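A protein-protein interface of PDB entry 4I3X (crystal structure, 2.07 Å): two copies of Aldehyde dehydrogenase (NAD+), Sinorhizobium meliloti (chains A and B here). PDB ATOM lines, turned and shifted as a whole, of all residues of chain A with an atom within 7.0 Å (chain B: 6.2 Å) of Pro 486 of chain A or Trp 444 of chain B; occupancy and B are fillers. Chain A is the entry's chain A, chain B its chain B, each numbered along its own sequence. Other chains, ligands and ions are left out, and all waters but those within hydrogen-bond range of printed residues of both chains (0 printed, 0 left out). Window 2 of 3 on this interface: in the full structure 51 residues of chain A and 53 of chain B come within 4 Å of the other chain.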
ATOM      1  N   ALA A 141     -16.193  23.287   9.152  1.00  0.00           N
ATOM      2  CA  ALA A 141     -16.200  24.721   9.131  1.00  0.00           C
ATOM      3  C   ALA A 141     -15.246  25.170  10.255  1.00  0.00           C
ATOM      4  O   ALA A 141     -15.662  25.361  11.383  1.00  0.00           O
ATOM      5  CB  ALA A 141     -17.627  25.231   9.360  1.00  0.00           C
ATOM      6  N   ARG A 142     -13.964  25.334   9.935  1.00  0.00           N
ATOM      7  CA  ARG A 142     -12.923  25.468  10.968  1.00  0.00           C
ATOM      8  C   ARG A 142     -11.744  26.158  10.294  1.00  0.00           C
ATOM      9  O   ARG A 142     -11.577  25.939   9.123  1.00  0.00           O
ATOM     10  CB  ARG A 142     -12.516  24.028  11.414  1.00  0.00           C
ATOM     11  CG  ARG A 142     -11.366  23.935  12.430  1.00  0.00           C
ATOM     12  CD  ARG A 142     -11.403  22.595  13.177  1.00  0.00           C
ATOM     13  NE  ARG A 142     -12.557  22.640  14.092  1.00  0.00           N
ATOM     14  CZ  ARG A 142     -12.497  23.012  15.365  1.00  0.00           C
ATOM     15  NH1 ARG A 142     -11.326  23.278  15.970  1.00  0.00           N
ATOM     16  NH2 ARG A 142     -13.613  23.050  16.078  1.00  0.00           N
ATOM     17  N   LYS A 143     -10.949  26.972  11.014  1.00  0.00           N
ATOM     18  CA  LYS A 143      -9.671  27.419  10.480  1.00  0.00           C
ATOM     19  C   LYS A 143      -8.538  26.857  11.346  1.00  0.00           C
ATOM     20  O   LYS A 143      -8.744  26.715  12.552  1.00  0.00           O
ATOM     21  CB  LYS A 143      -9.571  28.925  10.439  1.00  0.00           C
ATOM     22  CG  LYS A 143     -10.557  29.566   9.454  1.00  0.00           C
ATOM     23  CD  LYS A 143     -10.203  31.033   9.222  1.00  0.00           C
ATOM     24  CE  LYS A 143     -11.297  31.826   8.504  1.00  0.00           C
ATOM     25  NZ  LYS A 143     -11.696  31.230   7.208  1.00  0.00           N
ATOM     26  N   PHE A 145      -4.590  27.827  12.339  1.00  0.00           N
ATOM     27  CA  PHE A 145      -3.583  28.930  12.333  1.00  0.00           C
ATOM     28  C   PHE A 145      -2.256  28.368  12.839  1.00  0.00           C
ATOM     29  O   PHE A 145      -2.221  27.424  13.677  1.00  0.00           O
ATOM     30  CB  PHE A 145      -4.036  30.008  13.352  1.00  0.00           C
ATOM     31  CG  PHE A 145      -5.458  30.495  13.112  1.00  0.00           C
ATOM     32  CD1 PHE A 145      -6.527  29.736  13.572  1.00  0.00           C
ATOM     33  CD2 PHE A 145      -5.696  31.654  12.340  1.00  0.00           C
ATOM     34  CE1 PHE A 145      -7.835  30.155  13.355  1.00  0.00           C
ATOM     35  CE2 PHE A 145      -6.990  32.073  12.080  1.00  0.00           C
ATOM     36  CZ  PHE A 145      -8.064  31.336  12.609  1.00  0.00           C
ATOM     37  N   SER A 484      -6.604  25.208  16.073  1.00  0.00           N
ATOM     38  CA  SER A 484      -7.775  25.408  15.200  1.00  0.00           C
ATOM     39  C   SER A 484      -8.987  25.900  15.989  1.00  0.00           C
ATOM     40  O   SER A 484      -9.146  25.577  17.162  1.00  0.00           O
ATOM     41  CB  SER A 484      -8.090  24.123  14.492  1.00  0.00           C
ATOM     42  OG  SER A 484      -8.554  23.197  15.468  1.00  0.00           O
ATOM     43  N   LEU A 485      -9.820  26.712  15.321  1.00  0.00           N
ATOM     44  CA  LEU A 485     -11.009  27.350  15.960  1.00  0.00           C
ATOM     45  C   LEU A 485     -12.220  27.001  15.103  1.00  0.00           C
ATOM     46  O   LEU A 485     -12.085  27.005  13.865  1.00  0.00           O
ATOM     47  CB  LEU A 485     -10.846  28.878  16.003  1.00  0.00           C
ATOM     48  CG  LEU A 485      -9.636  29.515  16.740  1.00  0.00           C
ATOM     49  CD1 LEU A 485      -9.570  31.047  16.647  1.00  0.00           C
ATOM     50  CD2 LEU A 485      -9.636  29.104  18.190  1.00  0.00           C
ATOM     51  N   PRO A 486     -13.397  26.738  15.751  1.00  0.00           N
ATOM     52  CA  PRO A 486     -14.663  26.663  15.005  1.00  0.00           C
ATOM     53  C   PRO A 486     -14.813  27.904  14.149  1.00  0.00           C
ATOM     54  O   PRO A 486     -14.514  29.011  14.609  1.00  0.00           O
ATOM     55  CB  PRO A 486     -15.758  26.585  16.129  1.00  0.00           C
ATOM     56  CG  PRO A 486     -15.026  25.908  17.297  1.00  0.00           C
ATOM     57  CD  PRO A 486     -13.627  26.627  17.211  1.00  0.00           C
ATOM     58  N   TRP A 487     -15.216  27.720  12.889  1.00  0.00           N
ATOM     59  CA  TRP A 487     -15.488  28.885  12.039  1.00  0.00           C
ATOM     60  C   TRP A 487     -16.753  28.737  11.167  1.00  0.00           C
ATOM     61  O   TRP A 487     -16.639  28.643   9.949  1.00  0.00           O
ATOM     62  CB  TRP A 487     -14.271  29.209  11.148  1.00  0.00           C
ATOM     63  CG  TRP A 487     -14.244  30.682  10.801  1.00  0.00           C
ATOM     64  CD1 TRP A 487     -14.887  31.317   9.721  1.00  0.00           C
ATOM     65  CD2 TRP A 487     -13.626  31.729  11.575  1.00  0.00           C
ATOM     66  NE1 TRP A 487     -14.667  32.670   9.769  1.00  0.00           N
ATOM     67  CE2 TRP A 487     -13.914  32.984  10.883  1.00  0.00           C
ATOM     68  CE3 TRP A 487     -12.840  31.751  12.727  1.00  0.00           C
ATOM     69  CZ2 TRP A 487     -13.424  34.205  11.333  1.00  0.00           C
ATOM     70  CZ3 TRP A 487     -12.378  32.983  13.178  1.00  0.00           C
ATOM     71  CH2 TRP A 487     -12.674  34.188  12.494  1.00  0.00           C
ATOM     72  N   PRO A 488     -17.977  28.728  11.783  1.00  0.00           N
ATOM     73  CA  PRO A 488     -19.243  28.384  11.057  1.00  0.00           C
ATOM     74  C   PRO A 488     -19.648  29.503  10.099  1.00  0.00           C
ATOM     75  O   PRO A 488     -18.979  30.574  10.110  1.00  0.00           O
ATOM     76  CB  PRO A 488     -20.282  28.289  12.191  1.00  0.00           C
ATOM     77  CG  PRO A 488     -19.738  29.173  13.321  1.00  0.00           C
ATOM     78  CD  PRO A 488     -18.217  29.057  13.219  1.00  0.00           C
ATOM     79  N   LEU B 270     -18.708  24.911  30.696  1.00  0.00           N
ATOM     80  CA  LEU B 270     -19.663  24.353  29.733  1.00  0.00           C
ATOM     81  C   LEU B 270     -21.098  24.091  30.284  1.00  0.00           C
ATOM     82  O   LEU B 270     -21.253  23.665  31.400  1.00  0.00           O
ATOM     83  CB  LEU B 270     -19.121  23.048  29.136  1.00  0.00           C
ATOM     84  CG  LEU B 270     -17.811  23.208  28.276  1.00  0.00           C
ATOM     85  CD1 LEU B 270     -17.523  21.872  27.601  1.00  0.00           C
ATOM     86  CD2 LEU B 270     -18.010  24.350  27.265  1.00  0.00           C
ATOM     87  N   ASP B 273     -25.708  20.902  27.708  1.00  0.00           N
ATOM     88  CA  ASP B 273     -25.727  20.564  26.278  1.00  0.00           C
ATOM     89  C   ASP B 273     -24.317  20.551  25.699  1.00  0.00           C
ATOM     90  O   ASP B 273     -24.027  19.717  24.891  1.00  0.00           O
ATOM     91  CB  ASP B 273     -26.539  21.564  25.444  1.00  0.00           C
ATOM     92  CG  ASP B 273     -28.009  21.530  25.781  1.00  0.00           C
ATOM     93  OD1 ASP B 273     -28.414  20.647  26.554  1.00  0.00           O
ATOM     94  OD2 ASP B 273     -28.769  22.372  25.268  1.00  0.00           O
ATOM     95  N   ASP B 274     -23.478  21.502  26.079  1.00  0.00           N
ATOM     96  CA  ASP B 274     -22.078  21.469  25.647  1.00  0.00           C
ATOM     97  C   ASP B 274     -21.387  20.180  26.156  1.00  0.00           C
ATOM     98  O   ASP B 274     -20.580  19.598  25.459  1.00  0.00           O
ATOM     99  CB  ASP B 274     -21.325  22.661  26.244  1.00  0.00           C
ATOM    100  CG  ASP B 274     -21.623  24.004  25.562  1.00  0.00           C
ATOM    101  OD1 ASP B 274     -21.972  24.037  24.363  1.00  0.00           O
ATOM    102  OD2 ASP B 274     -21.445  25.053  26.266  1.00  0.00           O
ATOM    103  N   LEU B 275     -21.713  19.737  27.379  1.00  0.00           N
ATOM    104  CA  LEU B 275     -21.091  18.534  27.952  1.00  0.00           C
ATOM    105  C   LEU B 275     -21.444  17.296  27.159  1.00  0.00           C
ATOM    106  O   LEU B 275     -20.606  16.427  26.997  1.00  0.00           O
ATOM    107  CB  LEU B 275     -21.407  18.346  29.432  1.00  0.00           C
ATOM    108  CG  LEU B 275     -20.776  19.407  30.345  1.00  0.00           C
ATOM    109  CD1 LEU B 275     -21.404  19.380  31.758  1.00  0.00           C
ATOM    110  CD2 LEU B 275     -19.278  19.177  30.448  1.00  0.00           C
ATOM    111  N   ARG B 277     -21.923  17.386  23.949  1.00  0.00           N
ATOM    112  CA  ARG B 277     -21.187  17.452  22.696  1.00  0.00           C
ATOM    113  C   ARG B 277     -19.755  17.078  22.988  1.00  0.00           C
ATOM    114  O   ARG B 277     -19.144  16.417  22.173  1.00  0.00           O
ATOM    115  CB  ARG B 277     -21.233  18.854  22.063  1.00  0.00           C
ATOM    116  CG  ARG B 277     -22.641  19.258  21.597  1.00  0.00           C
ATOM    117  CD  ARG B 277     -22.619  20.384  20.570  1.00  0.00           C
ATOM    118  NE  ARG B 277     -22.173  21.659  21.133  1.00  0.00           N
ATOM    119  CZ  ARG B 277     -20.993  22.245  20.863  1.00  0.00           C
ATOM    120  NH1 ARG B 277     -20.108  21.671  20.044  1.00  0.00           N
ATOM    121  NH2 ARG B 277     -20.685  23.419  21.429  1.00  0.00           N
ATOM    122  N   ALA B 278     -19.235  17.509  24.143  1.00  0.00           N
ATOM    123  CA  ALA B 278     -17.864  17.140  24.598  1.00  0.00           C
ATOM    124  C   ALA B 278     -17.740  15.619  24.822  1.00  0.00           C
ATOM    125  O   ALA B 278     -16.713  14.988  24.480  1.00  0.00           O
ATOM    126  CB  ALA B 278     -17.476  17.974  25.835  1.00  0.00           C
ATOM    127  N   LEU B 281     -17.349  13.982  21.526  1.00  0.00           N
ATOM    128  CA  LEU B 281     -15.941  14.059  21.081  1.00  0.00           C
ATOM    129  C   LEU B 281     -15.079  13.098  21.926  1.00  0.00           C
ATOM    130  O   LEU B 281     -14.285  12.360  21.369  1.00  0.00           O
ATOM    131  CB  LEU B 281     -15.391  15.477  21.190  1.00  0.00           C
ATOM    132  CG  LEU B 281     -16.010  16.557  20.321  1.00  0.00           C
ATOM    133  CD1 LEU B 281     -15.517  17.918  20.785  1.00  0.00           C
ATOM    134  CD2 LEU B 281     -15.685  16.321  18.832  1.00  0.00           C
ATOM    135  N   GLY B 420      -6.928  18.631  22.555  1.00  0.00           N
ATOM    136  CA  GLY B 420      -8.302  19.127  22.281  1.00  0.00           C
ATOM    137  C   GLY B 420      -8.734  19.888  23.550  1.00  0.00           C
ATOM    138  O   GLY B 420      -8.511  19.409  24.648  1.00  0.00           O
ATOM    139  N   VAL B 421      -9.293  21.085  23.437  1.00  0.00           N
ATOM    140  CA  VAL B 421      -9.834  21.759  24.623  1.00  0.00           C
ATOM    141  C   VAL B 421     -11.281  22.179  24.383  1.00  0.00           C
ATOM    142  O   VAL B 421     -11.556  22.877  23.399  1.00  0.00           O
ATOM    143  CB  VAL B 421      -8.992  22.995  24.931  1.00  0.00           C
ATOM    144  CG1 VAL B 421      -9.467  23.741  26.189  1.00  0.00           C
ATOM    145  CG2 VAL B 421      -7.520  22.555  25.043  1.00  0.00           C
ATOM    146  N   CYS B 422     -12.203  21.816  25.268  1.00  0.00           N
ATOM    147  CA  CYS B 422     -13.607  22.280  25.078  1.00  0.00           C
ATOM    148  C   CYS B 422     -13.972  23.357  26.097  1.00  0.00           C
ATOM    149  O   CYS B 422     -13.880  23.103  27.311  1.00  0.00           O
ATOM    150  CB  CYS B 422     -14.580  21.100  25.196  1.00  0.00           C
ATOM    151  SG  CYS B 422     -14.263  19.768  23.990  1.00  0.00           S
ATOM    152  N   THR B 423     -14.377  24.530  25.601  1.00  0.00           N
ATOM    153  CA  THR B 423     -14.611  25.746  26.398  1.00  0.00           C
ATOM    154  C   THR B 423     -15.192  26.766  25.448  1.00  0.00           C
ATOM    155  O   THR B 423     -14.986  26.659  24.251  1.00  0.00           O
ATOM    156  CB  THR B 423     -13.298  26.308  27.027  1.00  0.00           C
ATOM    157  OG1 THR B 423     -13.578  27.429  27.891  1.00  0.00           O
ATOM    158  CG2 THR B 423     -12.349  26.806  25.953  1.00  0.00           C
ATOM    159  N   ASN B 424     -15.929  27.743  25.966  1.00  0.00           N
ATOM    160  CA  ASN B 424     -16.492  28.829  25.140  1.00  0.00           C
ATOM    161  C   ASN B 424     -15.888  30.186  25.449  1.00  0.00           C
ATOM    162  O   ASN B 424     -16.172  31.185  24.757  1.00  0.00           O
ATOM    163  CB  ASN B 424     -17.991  28.913  25.416  1.00  0.00           C
ATOM    164  CG  ASN B 424     -18.729  27.632  24.993  1.00  0.00           C
ATOM    165  OD1 ASN B 424     -18.462  27.048  23.937  1.00  0.00           O
ATOM    166  ND2 ASN B 424     -19.632  27.175  25.838  1.00  0.00           N
ATOM    167  N   MET B 429      -9.312  29.711  26.122  1.00  0.00           N
ATOM    168  CA  MET B 429      -8.841  29.123  24.889  1.00  0.00           C
ATOM    169  C   MET B 429      -7.399  29.578  24.620  1.00  0.00           C
ATOM    170  O   MET B 429      -6.544  28.743  24.438  1.00  0.00           O
ATOM    171  CB  MET B 429      -9.705  29.563  23.693  1.00  0.00           C
ATOM    172  CG  MET B 429     -11.028  28.849  23.553  1.00  0.00           C
ATOM    173  SD  MET B 429     -11.887  29.645  22.158  1.00  0.00           S
ATOM    174  CE  MET B 429     -13.517  28.824  22.331  1.00  0.00           C
ATOM    175  N   ASN B 442      -6.394  21.901  19.383  1.00  0.00           N
ATOM    176  CA  ASN B 442      -7.664  22.029  18.670  1.00  0.00           C
ATOM    177  C   ASN B 442      -8.741  22.485  19.668  1.00  0.00           C
ATOM    178  O   ASN B 442      -8.946  21.806  20.714  1.00  0.00           O
ATOM    179  CB  ASN B 442      -8.026  20.673  18.128  1.00  0.00           C
ATOM    180  CG  ASN B 442      -7.297  20.369  16.873  1.00  0.00           C
ATOM    181  OD1 ASN B 442      -7.005  21.289  16.128  1.00  0.00           O
ATOM    182  ND2 ASN B 442      -6.968  19.118  16.634  1.00  0.00           N
ATOM    183  N   ILE B 443      -9.404  23.617  19.392  1.00  0.00           N
ATOM    184  CA  ILE B 443     -10.515  24.081  20.259  1.00  0.00           C
ATOM    185  C   ILE B 443     -11.813  23.437  19.800  1.00  0.00           C
ATOM    186  O   ILE B 443     -12.174  23.522  18.609  1.00  0.00           O
ATOM    187  CB  ILE B 443     -10.641  25.597  20.250  1.00  0.00           C
ATOM    188  CG1 ILE B 443      -9.314  26.246  20.733  1.00  0.00           C
ATOM    189  CG2 ILE B 443     -11.913  26.086  21.018  1.00  0.00           C
ATOM    190  CD1 ILE B 443      -8.861  25.814  22.138  1.00  0.00           C
ATOM    191  N   TRP B 444     -12.463  22.694  20.690  1.00  0.00           N
ATOM    192  CA  TRP B 444     -13.728  22.060  20.354  1.00  0.00           C
ATOM    193  C   TRP B 444     -13.582  21.031  19.239  1.00  0.00           C
ATOM    194  O   TRP B 444     -14.501  20.807  18.409  1.00  0.00           O
ATOM    195  CB  TRP B 444     -14.777  23.119  19.982  1.00  0.00           C
ATOM    196  CG  TRP B 444     -15.657  23.460  21.160  1.00  0.00           C
ATOM    197  CD1 TRP B 444     -15.845  24.699  21.769  1.00  0.00           C
ATOM    198  CD2 TRP B 444     -16.491  22.520  21.918  1.00  0.00           C
ATOM    199  NE1 TRP B 444     -16.749  24.596  22.807  1.00  0.00           N
ATOM    200  CE2 TRP B 444     -17.180  23.305  22.933  1.00  0.00           C
ATOM    201  CE3 TRP B 444     -16.754  21.163  21.821  1.00  0.00           C
ATOM    202  CZ2 TRP B 444     -18.023  22.720  23.859  1.00  0.00           C
ATOM    203  CZ3 TRP B 444     -17.646  20.595  22.733  1.00  0.00           C
ATOM    204  CH2 TRP B 444     -18.253  21.363  23.743  1.00  0.00           C
ATOM    205  N   GLU B 445     -12.435  20.385  19.218  1.00  0.00           N
ATOM    206  CA  GLU B 445     -12.258  19.167  18.425  1.00  0.00           C
ATOM    207  C   GLU B 445     -11.349  18.227  19.208  1.00  0.00           C
ATOM    208  O   GLU B 445     -10.709  18.659  20.152  1.00  0.00           O
ATOM    209  CB  GLU B 445     -11.668  19.488  17.046  1.00  0.00           C
ATOM    210  CG  GLU B 445     -12.652  19.350  15.900  1.00  0.00           C
ATOM    211  CD  GLU B 445     -13.269  17.936  15.800  1.00  0.00           C
ATOM    212  OE1 GLU B 445     -12.695  16.928  16.303  1.00  0.00           O
ATOM    213  OE2 GLU B 445     -14.380  17.829  15.219  1.00  0.00           O
ATOM    214  N   VAL B 446     -11.280  16.974  18.780  1.00  0.00           N
ATOM    215  CA  VAL B 446     -10.426  15.992  19.396  1.00  0.00           C
ATOM    216  C   VAL B 446      -8.983  16.296  18.935  1.00  0.00           C
ATOM    217  O   VAL B 446      -8.766  16.924  17.868  1.00  0.00           O
ATOM    218  CB  VAL B 446     -10.810  14.572  18.953  1.00  0.00           C
ATOM    219  CG1 VAL B 446     -12.180  14.174  19.515  1.00  0.00           C
ATOM    220  CG2 VAL B 446     -10.748  14.423  17.413  1.00  0.00           C
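The backbone carbonyl oxygen (O) of Ser 484 of chain A is in hydrogen-bond range of the backbone NH (N) of Ile 443 of chain B, at 3.0 Å. NH1 of Arg 142 of chain A is in hydrogen-bond range of O of Ile 443 of chain B. The side-chain hydroxyl of Ser 484 of chain A lies within hydrogen-bond range of the side-chain amide oxygen of Asn 442 of chain B. The guanidinium group of Arg 142 of chain A lies within hydrogen-bond range of the backbone carbonyl oxygen of Trp 444 of chain B (3.4 Å).
The side-chain amide nitrogen (ND2) of Asn 442 of chain B sits at hydrogen-bond distance from the backbone carbonyl oxygen (O) of Val 446 of chain B, 3.1 Å away. N of Val 421 of chain B lies within hydrogen-bond range of O of Asn 442 of chain B (2.8 Å). NE1 of Trp 444 of chain B lies within hydrogen-bond range of OD1 of Asn 424 of chain B. O of Lys 143 of chain A sits at hydrogen-bond distance from N of Leu 485 of chain A, 3.0 Å away. O of Thr 423 of chain B lies within hydrogen-bond range of NE1 of Trp 444 of chain B (3.1 Å). The backbone NH (N) of Trp 444 of chain B lies within hydrogen-bond range of the backbone carbonyl oxygen (O) of Val 421 of chain B.
Among the printed residues, pairs that only touch across the chains: Arg 142 of chain A with Glu 445 of chain B (3.7 Å), Leu 485 of chain A with Ile 443 of chain B (3.8 Å), Pro 486 of chain A with Ile 443 of chain B (3.7 Å) and Pro 486 of chain A with Trp 444 of chain B (3.9 Å).
Pro 486 of chain A touches two residues of chain B. Trp 444 of chain B touches just these residues of chain A: Arg 142 and Pro 486. Printed residues of chain B within 4 Å of Leu 485 of chain A: Ile 443 (3.8 Å). Of the printed residues of chain B, Arg 142 of chain A touches Ile 443 (2.8 Å), Trp 444 (3.4 Å) and Glu 445 (3.7 Å). Arg 277 of chain B touches none of the printed residues of chain A. Trp 487 of chain A touches none of the printed residues of chain B. The nearest printed residue of chain A that does not touch Ile 443 of chain B is Lys 143 of chain A (7.5 Å).
Of the 18 printed residues of chain B, 4 touch a printed residue of chain A. Hydrophobic or aromatic side chains of chain B within 4 Å of the printed part of chain A: Ile 443 and Trp 444. Along chain B the printed residues that touch a printed residue of chain A span positions 442 to 445. Of the 9 printed residues of chain A, 4 touch a printed residue of chain B. Among the printed residues, 8 pairs touch across the chains. Among the printed residues, no Asp or Glu carboxylate lies within 4 Å of a Lys or Arg side-chain nitrogen of the other chain.
No position is printed for both chains.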
